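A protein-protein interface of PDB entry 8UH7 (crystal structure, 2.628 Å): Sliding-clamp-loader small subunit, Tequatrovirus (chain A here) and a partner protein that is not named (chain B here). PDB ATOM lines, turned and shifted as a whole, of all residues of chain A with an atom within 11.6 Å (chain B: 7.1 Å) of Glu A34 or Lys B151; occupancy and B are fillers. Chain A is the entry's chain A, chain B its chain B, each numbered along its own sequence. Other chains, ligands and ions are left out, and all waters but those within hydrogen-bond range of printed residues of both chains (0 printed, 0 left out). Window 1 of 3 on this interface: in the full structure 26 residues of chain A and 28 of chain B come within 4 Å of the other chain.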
ATOM      1  N   GLN A  26       4.882  29.847 -19.656  1.00  0.00           N
ATOM      2  CA  GLN A  26       4.169  28.593 -19.430  1.00  0.00           C
ATOM      3  C   GLN A  26       3.514  28.092 -20.710  1.00  0.00           C
ATOM      4  O   GLN A  26       3.548  26.891 -21.005  1.00  0.00           O
ATOM      5  CB  GLN A  26       3.122  28.774 -18.330  1.00  0.00           C
ATOM      6  CG  GLN A  26       2.339  27.511 -18.000  1.00  0.00           C
ATOM      7  CD  GLN A  26       3.190  26.460 -17.317  1.00  0.00           C
ATOM      8  OE1 GLN A  26       3.742  26.694 -16.241  1.00  0.00           O
ATOM      9  NE2 GLN A  26       3.303  25.292 -17.940  1.00  0.00           N
ATOM     10  N   SER A  27       2.909  28.996 -21.483  1.00  0.00           N
ATOM     11  CA  SER A  27       2.314  28.582 -22.751  1.00  0.00           C
ATOM     12  C   SER A  27       3.381  28.104 -23.734  1.00  0.00           C
ATOM     13  O   SER A  27       3.192  27.096 -24.427  1.00  0.00           O
ATOM     14  CB  SER A  27       1.496  29.728 -23.347  1.00  0.00           C
ATOM     15  OG  SER A  27       2.282  30.897 -23.496  1.00  0.00           O
ATOM     16  N   ALA A  28       4.519  28.802 -23.792  1.00  0.00           N
ATOM     17  CA  ALA A  28       5.601  28.384 -24.678  1.00  0.00           C
ATOM     18  C   ALA A  28       6.160  27.024 -24.278  1.00  0.00           C
ATOM     19  O   ALA A  28       6.580  26.247 -25.143  1.00  0.00           O
ATOM     20  CB  ALA A  28       6.711  29.433 -24.681  1.00  0.00           C
ATOM     21  N   ALA A  29       6.180  26.721 -22.981  1.00  0.00           N
ATOM     22  CA  ALA A  29       6.659  25.419 -22.531  1.00  0.00           C
ATOM     23  C   ALA A  29       5.637  24.322 -22.810  1.00  0.00           C
ATOM     24  O   ALA A  29       6.008  23.209 -23.196  1.00  0.00           O
ATOM     25  CB  ALA A  29       7.001  25.466 -21.045  1.00  0.00           C
ATOM     26  N   ASP A  30       4.348  24.619 -22.616  1.00  0.00           N
ATOM     27  CA  ASP A  30       3.298  23.674 -22.981  1.00  0.00           C
ATOM     28  C   ASP A  30       3.240  23.443 -24.483  1.00  0.00           C
ATOM     29  O   ASP A  30       2.657  22.448 -24.923  1.00  0.00           O
ATOM     30  CB  ASP A  30       1.939  24.163 -22.476  1.00  0.00           C
ATOM     31  CG  ASP A  30       1.880  24.265 -20.962  1.00  0.00           C
ATOM     32  OD1 ASP A  30       2.672  23.571 -20.288  1.00  0.00           O
ATOM     33  OD2 ASP A  30       1.041  25.036 -20.446  1.00  0.00           O
ATOM     34  N   SER A  31       3.812  24.351 -25.277  1.00  0.00           N
ATOM     35  CA  SER A  31       3.965  24.086 -26.705  1.00  0.00           C
ATOM     36  C   SER A  31       4.722  22.789 -26.961  1.00  0.00           C
ATOM     37  O   SER A  31       4.502  22.135 -27.989  1.00  0.00           O
ATOM     38  CB  SER A  31       4.681  25.254 -27.383  1.00  0.00           C
ATOM     39  OG  SER A  31       5.215  24.861 -28.635  1.00  0.00           O
ATOM     40  N   PHE A  32       5.614  22.401 -26.049  1.00  0.00           N
ATOM     41  CA  PHE A  32       6.409  21.184 -26.177  1.00  0.00           C
ATOM     42  C   PHE A  32       5.812  20.013 -25.403  1.00  0.00           C
ATOM     43  O   PHE A  32       6.541  19.102 -24.999  1.00  0.00           O
ATOM     44  CB  PHE A  32       7.844  21.438 -25.714  1.00  0.00           C
ATOM     45  CG  PHE A  32       8.570  22.479 -26.521  1.00  0.00           C
ATOM     46  CD1 PHE A  32       9.095  22.168 -27.765  1.00  0.00           C
ATOM     47  CD2 PHE A  32       8.737  23.764 -26.032  1.00  0.00           C
ATOM     48  CE1 PHE A  32       9.767  23.119 -28.509  1.00  0.00           C
ATOM     49  CE2 PHE A  32       9.410  24.720 -26.771  1.00  0.00           C
ATOM     50  CZ  PHE A  32       9.924  24.397 -28.012  1.00  0.00           C
ATOM     51  N   LYS A  33       4.493  20.015 -25.190  1.00  0.00           N
ATOM     52  CA  LYS A  33       3.836  19.013 -24.357  1.00  0.00           C
ATOM     53  C   LYS A  33       3.433  17.771 -25.136  1.00  0.00           C
ATOM     54  O   LYS A  33       2.412  17.148 -24.817  1.00  0.00           O
ATOM     55  CB  LYS A  33       2.624  19.626 -23.654  1.00  0.00           C
ATOM     56  CG  LYS A  33       2.400  19.136 -22.234  1.00  0.00           C
ATOM     57  CD  LYS A  33       1.510  20.104 -21.467  1.00  0.00           C
ATOM     58  CE  LYS A  33       1.475  19.770 -19.983  1.00  0.00           C
ATOM     59  NZ  LYS A  33       0.893  20.873 -19.163  1.00  0.00           N
ATOM     60  N   GLU A  34       4.198  17.414 -26.164  1.00  0.00           N
ATOM     61  CA  GLU A  34       4.017  16.131 -26.826  1.00  0.00           C
ATOM     62  C   GLU A  34       4.189  15.007 -25.813  1.00  0.00           C
ATOM     63  O   GLU A  34       5.140  15.006 -25.025  1.00  0.00           O
ATOM     64  CB  GLU A  34       5.021  15.994 -27.970  1.00  0.00           C
ATOM     65  CG  GLU A  34       5.704  14.643 -28.075  1.00  0.00           C
ATOM     66  CD  GLU A  34       6.933  14.686 -28.961  1.00  0.00           C
ATOM     67  OE1 GLU A  34       7.421  15.800 -29.248  1.00  0.00           O
ATOM     68  OE2 GLU A  34       7.413  13.608 -29.369  1.00  0.00           O
ATOM     69  N   LYS A  35       3.253  14.063 -25.812  1.00  0.00           N
ATOM     70  CA  LYS A  35       3.220  13.057 -24.762  1.00  0.00           C
ATOM     71  C   LYS A  35       2.874  11.688 -25.333  1.00  0.00           C
ATOM     72  O   LYS A  35       2.224  11.574 -26.377  1.00  0.00           O
ATOM     73  CB  LYS A  35       2.228  13.436 -23.654  1.00  0.00           C
ATOM     74  CG  LYS A  35       2.712  14.569 -22.752  1.00  0.00           C
ATOM     75  CD  LYS A  35       2.000  14.556 -21.404  1.00  0.00           C
ATOM     76  CE  LYS A  35       2.444  15.712 -20.516  1.00  0.00           C
ATOM     77  NZ  LYS A  35       1.809  15.639 -19.170  1.00  0.00           N
ATOM     78  N   ALA A  36       3.339  10.659 -24.608  1.00  0.00           N
ATOM     79  CA  ALA A  36       3.154   9.224 -24.828  1.00  0.00           C
ATOM     80  C   ALA A  36       4.276   8.651 -25.688  1.00  0.00           C
ATOM     81  O   ALA A  36       4.160   8.582 -26.916  1.00  0.00           O
ATOM     82  CB  ALA A  36       1.786   8.905 -25.441  1.00  0.00           C
ATOM     83  N   GLU A  37       5.366   8.236 -25.044  1.00  0.00           N
ATOM     84  CA  GLU A  37       6.509   7.621 -25.707  1.00  0.00           C
ATOM     85  C   GLU A  37       6.682   6.197 -25.202  1.00  0.00           C
ATOM     86  O   GLU A  37       6.575   5.936 -23.999  1.00  0.00           O
ATOM     87  CB  GLU A  37       7.803   8.420 -25.467  1.00  0.00           C
ATOM     88  CG  GLU A  37       8.066   8.770 -24.006  1.00  0.00           C
ATOM     89  CD  GLU A  37       9.548   8.848 -23.667  1.00  0.00           C
ATOM     90  OE1 GLU A  37      10.385   8.570 -24.551  1.00  0.00           O
ATOM     91  OE2 GLU A  37       9.875   9.180 -22.507  1.00  0.00           O
ATOM     92  N   ASN A  38       6.960   5.276 -26.120  1.00  0.00           N
ATOM     93  CA  ASN A  38       7.014   3.869 -25.751  1.00  0.00           C
ATOM     94  C   ASN A  38       7.836   3.108 -26.781  1.00  0.00           C
ATOM     95  O   ASN A  38       7.820   3.432 -27.970  1.00  0.00           O
ATOM     96  CB  ASN A  38       5.604   3.278 -25.648  1.00  0.00           C
ATOM     97  CG  ASN A  38       5.490   2.205 -24.582  1.00  0.00           C
ATOM     98  OD1 ASN A  38       6.408   1.994 -23.793  1.00  0.00           O
ATOM     99  ND2 ASN A  38       4.344   1.529 -24.548  1.00  0.00           N
ATOM    100  N   GLU A  39       8.557   2.094 -26.307  1.00  0.00           N
ATOM    101  CA  GLU A  39       9.226   1.140 -27.189  1.00  0.00           C
ATOM    102  C   GLU A  39       9.081  -0.276 -26.649  1.00  0.00           C
ATOM    103  O   GLU A  39      10.027  -1.072 -26.674  1.00  0.00           O
ATOM    104  CB  GLU A  39      10.696   1.497 -27.389  1.00  0.00           C
ATOM    105  CG  GLU A  39      10.914   2.602 -28.406  1.00  0.00           C
ATOM    106  CD  GLU A  39      12.225   2.462 -29.145  1.00  0.00           C
ATOM    107  OE1 GLU A  39      13.039   1.600 -28.757  1.00  0.00           O
ATOM    108  OE2 GLU A  39      12.434   3.212 -30.121  1.00  0.00           O
ATOM    109  N   PHE A  40       7.883  -0.613 -26.165  1.00  0.00           N
ATOM    110  CA  PHE A  40       7.632  -1.968 -25.689  1.00  0.00           C
ATOM    111  C   PHE A  40       7.669  -2.980 -26.823  1.00  0.00           C
ATOM    112  O   PHE A  40       8.096  -4.122 -26.618  1.00  0.00           O
ATOM    113  CB  PHE A  40       6.284  -2.040 -24.974  1.00  0.00           C
ATOM    114  CG  PHE A  40       6.344  -1.620 -23.536  1.00  0.00           C
ATOM    115  CD1 PHE A  40       7.473  -1.874 -22.777  1.00  0.00           C
ATOM    116  CD2 PHE A  40       5.271  -0.980 -22.940  1.00  0.00           C
ATOM    117  CE1 PHE A  40       7.533  -1.498 -21.452  1.00  0.00           C
ATOM    118  CE2 PHE A  40       5.328  -0.597 -21.614  1.00  0.00           C
ATOM    119  CZ  PHE A  40       6.461  -0.857 -20.872  1.00  0.00           C
ATOM    120  N   GLU A  42       9.601  -3.248 -29.256  1.00  0.00           N
ATOM    121  CA  GLU A  42      10.920  -3.778 -29.577  1.00  0.00           C
ATOM    122  C   GLU A  42      11.234  -5.014 -28.747  1.00  0.00           C
ATOM    123  O   GLU A  42      12.001  -5.877 -29.190  1.00  0.00           O
ATOM    124  CB  GLU A  42      12.000  -2.715 -29.367  1.00  0.00           C
ATOM    125  CG  GLU A  42      12.122  -1.706 -30.499  1.00  0.00           C
ATOM    126  CD  GLU A  42      13.536  -1.171 -30.645  1.00  0.00           C
ATOM    127  OE1 GLU A  42      14.032  -1.095 -31.789  1.00  0.00           O
ATOM    128  OE2 GLU A  42      14.158  -0.839 -29.612  1.00  0.00           O
ATOM    129  N   GLN B 123      11.492  20.465 -17.427  1.00  0.00           N
ATOM    130  CA  GLN B 123      12.201  20.183 -18.672  1.00  0.00           C
ATOM    131  C   GLN B 123      11.562  20.909 -19.850  1.00  0.00           C
ATOM    132  O   GLN B 123      12.266  21.498 -20.680  1.00  0.00           O
ATOM    133  CB  GLN B 123      12.239  18.678 -18.928  1.00  0.00           C
ATOM    134  CG  GLN B 123      13.021  17.897 -17.894  1.00  0.00           C
ATOM    135  CD  GLN B 123      13.143  16.433 -18.253  1.00  0.00           C
ATOM    136  OE1 GLN B 123      12.531  15.966 -19.213  1.00  0.00           O
ATOM    137  NE2 GLN B 123      13.938  15.699 -17.484  1.00  0.00           N
ATOM    138  N   ARG B 124      10.227  20.896 -19.928  1.00  0.00           N
ATOM    139  CA  ARG B 124       9.549  21.647 -20.979  1.00  0.00           C
ATOM    140  C   ARG B 124       9.955  23.114 -20.937  1.00  0.00           C
ATOM    141  O   ARG B 124      10.351  23.688 -21.961  1.00  0.00           O
ATOM    142  CB  ARG B 124       8.032  21.495 -20.852  1.00  0.00           C
ATOM    143  CG  ARG B 124       7.493  20.177 -21.387  1.00  0.00           C
ATOM    144  CD  ARG B 124       5.971  20.168 -21.417  1.00  0.00           C
ATOM    145  NE  ARG B 124       5.386  20.121 -20.080  1.00  0.00           N
ATOM    146  CZ  ARG B 124       5.063  18.998 -19.446  1.00  0.00           C
ATOM    147  NH1 ARG B 124       5.269  17.823 -20.027  1.00  0.00           N
ATOM    148  NH2 ARG B 124       4.534  19.047 -18.233  1.00  0.00           N
ATOM    149  N   ARG B 127      13.270  23.574 -22.409  1.00  0.00           N
ATOM    150  CA  ARG B 127      13.247  23.607 -23.867  1.00  0.00           C
ATOM    151  C   ARG B 127      12.973  25.017 -24.369  1.00  0.00           C
ATOM    152  O   ARG B 127      13.700  25.537 -25.224  1.00  0.00           O
ATOM    153  CB  ARG B 127      12.204  22.627 -24.398  1.00  0.00           C
ATOM    154  CG  ARG B 127      12.150  22.553 -25.912  1.00  0.00           C
ATOM    155  CD  ARG B 127      13.477  22.101 -26.492  1.00  0.00           C
ATOM    156  NE  ARG B 127      13.375  21.801 -27.917  1.00  0.00           N
ATOM    157  CZ  ARG B 127      13.610  22.681 -28.884  1.00  0.00           C
ATOM    158  NH1 ARG B 127      13.965  23.923 -28.584  1.00  0.00           N
ATOM    159  NH2 ARG B 127      13.492  22.318 -30.153  1.00  0.00           N
ATOM    160  N   ILE B 146      17.302   7.568 -20.111  1.00  0.00           N
ATOM    161  CA  ILE B 146      17.104   8.541 -21.185  1.00  0.00           C
ATOM    162  C   ILE B 146      15.627   8.871 -21.355  1.00  0.00           C
ATOM    163  O   ILE B 146      15.271   9.986 -21.758  1.00  0.00           O
ATOM    164  CB  ILE B 146      17.726   8.018 -22.497  1.00  0.00           C
ATOM    165  CG1 ILE B 146      17.571   9.044 -23.624  1.00  0.00           C
ATOM    166  CG2 ILE B 146      17.110   6.685 -22.897  1.00  0.00           C
ATOM    167  CD1 ILE B 146      18.310  10.340 -23.379  1.00  0.00           C
ATOM    168  N   ASP B 147      14.741   7.925 -21.034  1.00  0.00           N
ATOM    169  CA  ASP B 147      13.311   8.188 -21.122  1.00  0.00           C
ATOM    170  C   ASP B 147      12.846   9.199 -20.085  1.00  0.00           C
ATOM    171  O   ASP B 147      11.743   9.738 -20.214  1.00  0.00           O
ATOM    172  CB  ASP B 147      12.532   6.882 -20.975  1.00  0.00           C
ATOM    173  CG  ASP B 147      12.928   5.855 -22.018  1.00  0.00           C
ATOM    174  OD1 ASP B 147      13.136   6.246 -23.188  1.00  0.00           O
ATOM    175  OD2 ASP B 147      13.042   4.661 -21.664  1.00  0.00           O
ATOM    176  N   ILE B 149      14.169  12.021 -19.910  1.00  0.00           N
ATOM    177  CA  ILE B 149      14.332  13.277 -20.632  1.00  0.00           C
ATOM    178  C   ILE B 149      13.258  13.341 -21.709  1.00  0.00           C
ATOM    179  O   ILE B 149      13.081  12.384 -22.475  1.00  0.00           O
ATOM    180  CB  ILE B 149      15.736  13.390 -21.250  1.00  0.00           C
ATOM    181  CG1 ILE B 149      16.811  12.972 -20.246  1.00  0.00           C
ATOM    182  CG2 ILE B 149      15.993  14.808 -21.722  1.00  0.00           C
ATOM    183  CD1 ILE B 149      16.891  13.858 -19.020  1.00  0.00           C
ATOM    184  N   ILE B 150      12.538  14.467 -21.773  1.00  0.00           N
ATOM    185  CA  ILE B 150      11.441  14.578 -22.729  1.00  0.00           C
ATOM    186  C   ILE B 150      11.981  14.526 -24.157  1.00  0.00           C
ATOM    187  O   ILE B 150      13.163  14.784 -24.420  1.00  0.00           O
ATOM    188  CB  ILE B 150      10.623  15.860 -22.501  1.00  0.00           C
ATOM    189  CG1 ILE B 150      11.524  17.093 -22.592  1.00  0.00           C
ATOM    190  CG2 ILE B 150       9.913  15.806 -21.158  1.00  0.00           C
ATOM    191  CD1 ILE B 150      10.799  18.397 -22.338  1.00  0.00           C
ATOM    192  N   LYS B 151      11.095  14.179 -25.089  1.00  0.00           N
ATOM    193  CA  LYS B 151      11.513  14.021 -26.479  1.00  0.00           C
ATOM    194  C   LYS B 151      12.009  15.314 -27.120  1.00  0.00           C
ATOM    195  O   LYS B 151      12.980  15.244 -27.896  1.00  0.00           O
ATOM    196  CB  LYS B 151      10.368  13.408 -27.296  1.00  0.00           C
ATOM    197  CG  LYS B 151       9.819  12.105 -26.722  1.00  0.00           C
ATOM    198  CD  LYS B 151      10.908  11.048 -26.566  1.00  0.00           C
ATOM    199  CE  LYS B 151      11.482  10.628 -27.912  1.00  0.00           C
ATOM    200  NZ  LYS B 151      12.526   9.574 -27.768  1.00  0.00           N
ATOM    201  N   PRO B 152      11.411  16.491 -26.881  1.00  0.00           N
ATOM    202  CA  PRO B 152      11.999  17.719 -27.451  1.00  0.00           C
ATOM    203  C   PRO B 152      13.427  17.985 -26.997  1.00  0.00           C
ATOM    204  O   PRO B 152      14.254  18.430 -27.805  1.00  0.00           O
ATOM    205  CB  PRO B 152      11.034  18.813 -26.977  1.00  0.00           C
ATOM    206  CG  PRO B 152       9.733  18.111 -26.848  1.00  0.00           C
ATOM    207  CD  PRO B 152      10.072  16.749 -26.318  1.00  0.00           C
ATOM    208  N   LEU B 153      13.744  17.729 -25.724  1.00  0.00           N
ATOM    209  CA  LEU B 153      15.121  17.885 -25.264  1.00  0.00           C
ATOM    210  C   LEU B 153      16.055  16.919 -25.983  1.00  0.00           C
ATOM    211  O   LEU B 153      17.156  17.302 -26.395  1.00  0.00           O
ATOM    212  CB  LEU B 153      15.203  17.678 -23.752  1.00  0.00           C
ATOM    213  CG  LEU B 153      14.765  18.833 -22.851  1.00  0.00           C
ATOM    214  CD1 LEU B 153      14.871  18.432 -21.392  1.00  0.00           C
ATOM    215  CD2 LEU B 153      15.607  20.062 -23.125  1.00  0.00           C
ATOM    216  N   GLN B 154      15.632  15.661 -26.145  1.00  0.00           N
ATOM    217  CA  GLN B 154      16.456  14.689 -26.858  1.00  0.00           C
ATOM    218  C   GLN B 154      16.667  15.104 -28.309  1.00  0.00           C
ATOM    219  O   GLN B 154      17.737  14.869 -28.882  1.00  0.00           O
ATOM    220  CB  GLN B 154      15.817  13.301 -26.797  1.00  0.00           C
ATOM    221  CG  GLN B 154      15.534  12.786 -25.396  1.00  0.00           C
ATOM    222  CD  GLN B 154      15.013  11.359 -25.394  1.00  0.00           C
ATOM    223  OE1 GLN B 154      15.315  10.571 -26.294  1.00  0.00           O
ATOM    224  NE2 GLN B 154      14.222  11.019 -24.381  1.00  0.00           N
ATOM    225  N   SER B 155      15.654  15.721 -28.920  1.00  0.00           N
ATOM    226  CA  SER B 155      15.756  16.090 -30.327  1.00  0.00           C
ATOM    227  C   SER B 155      16.616  17.331 -30.520  1.00  0.00           C
ATOM    228  O   SER B 155      17.328  17.446 -31.524  1.00  0.00           O
ATOM    229  CB  SER B 155      14.362  16.315 -30.913  1.00  0.00           C
ATOM    230  OG  SER B 155      13.732  17.424 -30.299  1.00  0.00           O
ATOM    231  N   ARG B 156      16.566  18.267 -29.573  1.00  0.00           N
ATOM    232  CA  ARG B 156      17.320  19.507 -29.713  1.00  0.00           C
ATOM    233  C   ARG B 156      18.806  19.316 -29.435  1.00  0.00           C
ATOM    234  O   ARG B 156      19.621  20.127 -29.893  1.00  0.00           O
ATOM    235  CB  ARG B 156      16.728  20.568 -28.782  1.00  0.00           C
ATOM    236  CG  ARG B 156      17.421  21.921 -28.804  1.00  0.00           C
ATOM    237  CD  ARG B 156      17.305  22.612 -30.150  1.00  0.00           C
ATOM    238  NE  ARG B 156      17.602  24.038 -30.042  1.00  0.00           N
ATOM    239  CZ  ARG B 156      18.825  24.556 -30.105  1.00  0.00           C
ATOM    240  NH1 ARG B 156      19.875  23.763 -30.279  1.00  0.00           N
ATOM    241  NH2 ARG B 156      18.999  25.868 -29.994  1.00  0.00           N
ATOM    242  N   CYS B 157      19.182  18.260 -28.721  1.00  0.00           N
ATOM    243  CA  CYS B 157      20.559  18.044 -28.305  1.00  0.00           C
ATOM    244  C   CYS B 157      21.195  16.896 -29.079  1.00  0.00           C
ATOM    245  O   CYS B 157      20.514  16.069 -29.694  1.00  0.00           O
ATOM    246  CB  CYS B 157      20.636  17.745 -26.804  1.00  0.00           C
ATOM    247  SG  CYS B 157      19.891  18.994 -25.741  1.00  0.00           S
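NZ of Lys A33 lies within salt-bridge range of OD1 of Asp A30 (3.4 Å). The guanidinium group (NE) of Arg B127 is in hydrogen-bond range of the backbone carbonyl oxygen (O) of Pro B152 (3.5 Å). The side-chain amino group of Lys B151 lies within hydrogen-bond range of the side-chain amide oxygen of Gln B154 (3.3 Å). The side-chain hydroxyl of Ser B155 is in hydrogen-bond range of the backbone carbonyl oxygen of Lys B151, at 3.3 Å. The backbone carbonyl oxygen (O) of Pro B152 lies within hydrogen-bond range of the side-chain hydroxyl (OG) of Ser B155.
Among the printed residues, pairs that only touch across the chains: Ala A29 with Arg B124, Lys A35 with Arg B124, Phe A32 with Arg B127, Lys A33 with Arg B124, Glu A34 with Lys B151, Phe A32 with Arg B124 and Phe A32 with Pro B152.
The side-chain carboxylate (OE1) of Glu A37 lies within salt-bridge range of the side-chain amino group (NZ) of Lys B151. The side-chain carboxylate of Glu A37 lies close to the backbone carbonyl oxygen of Asp B147 (3.0 Å).
Of chain B, only Lys B151 (3.6 Å) comes within 4 Å of Glu A34. Of chain A, only Glu A34 (3.6 Å) and Glu A37 (3.2 Å) come within 4 Å of Lys B151. No residue of chain A comes within 4 Å of Ile B150. Pro B152 touches just one residue of chain A: Phe A32 (3.8 Å). No residue of chain A comes within 4 Å of Leu B153. No residue of chain A comes within 4 Å of Gln B154. No residue of chain A comes within 4 Å of Ser B155. Of the printed residues of chain A, Asp B147 touches Glu A37 (3.0 Å). Printed residues of chain A within 4 Å of Arg B127: Phe A32. Asp A30 touches none of the printed residues of chain B. The nearest residue of chain B that does not touch Glu A34 is Pro B152 (4.1 Å). The nearest residue of chain A that does not touch Lys B151 is Ala A36 (6.6 Å). The nearest printed residue of chain A that does not touch Arg B127 is Ala A29 (6.3 Å).
Of the 14 printed residues of chain B, 5 touch a printed residue of chain A. Hydrophobic or aromatic side chains of chain B within 4 Å of the printed part of chain A: Pro B152. Among the printed residues, 9 pairs touch across the chains.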
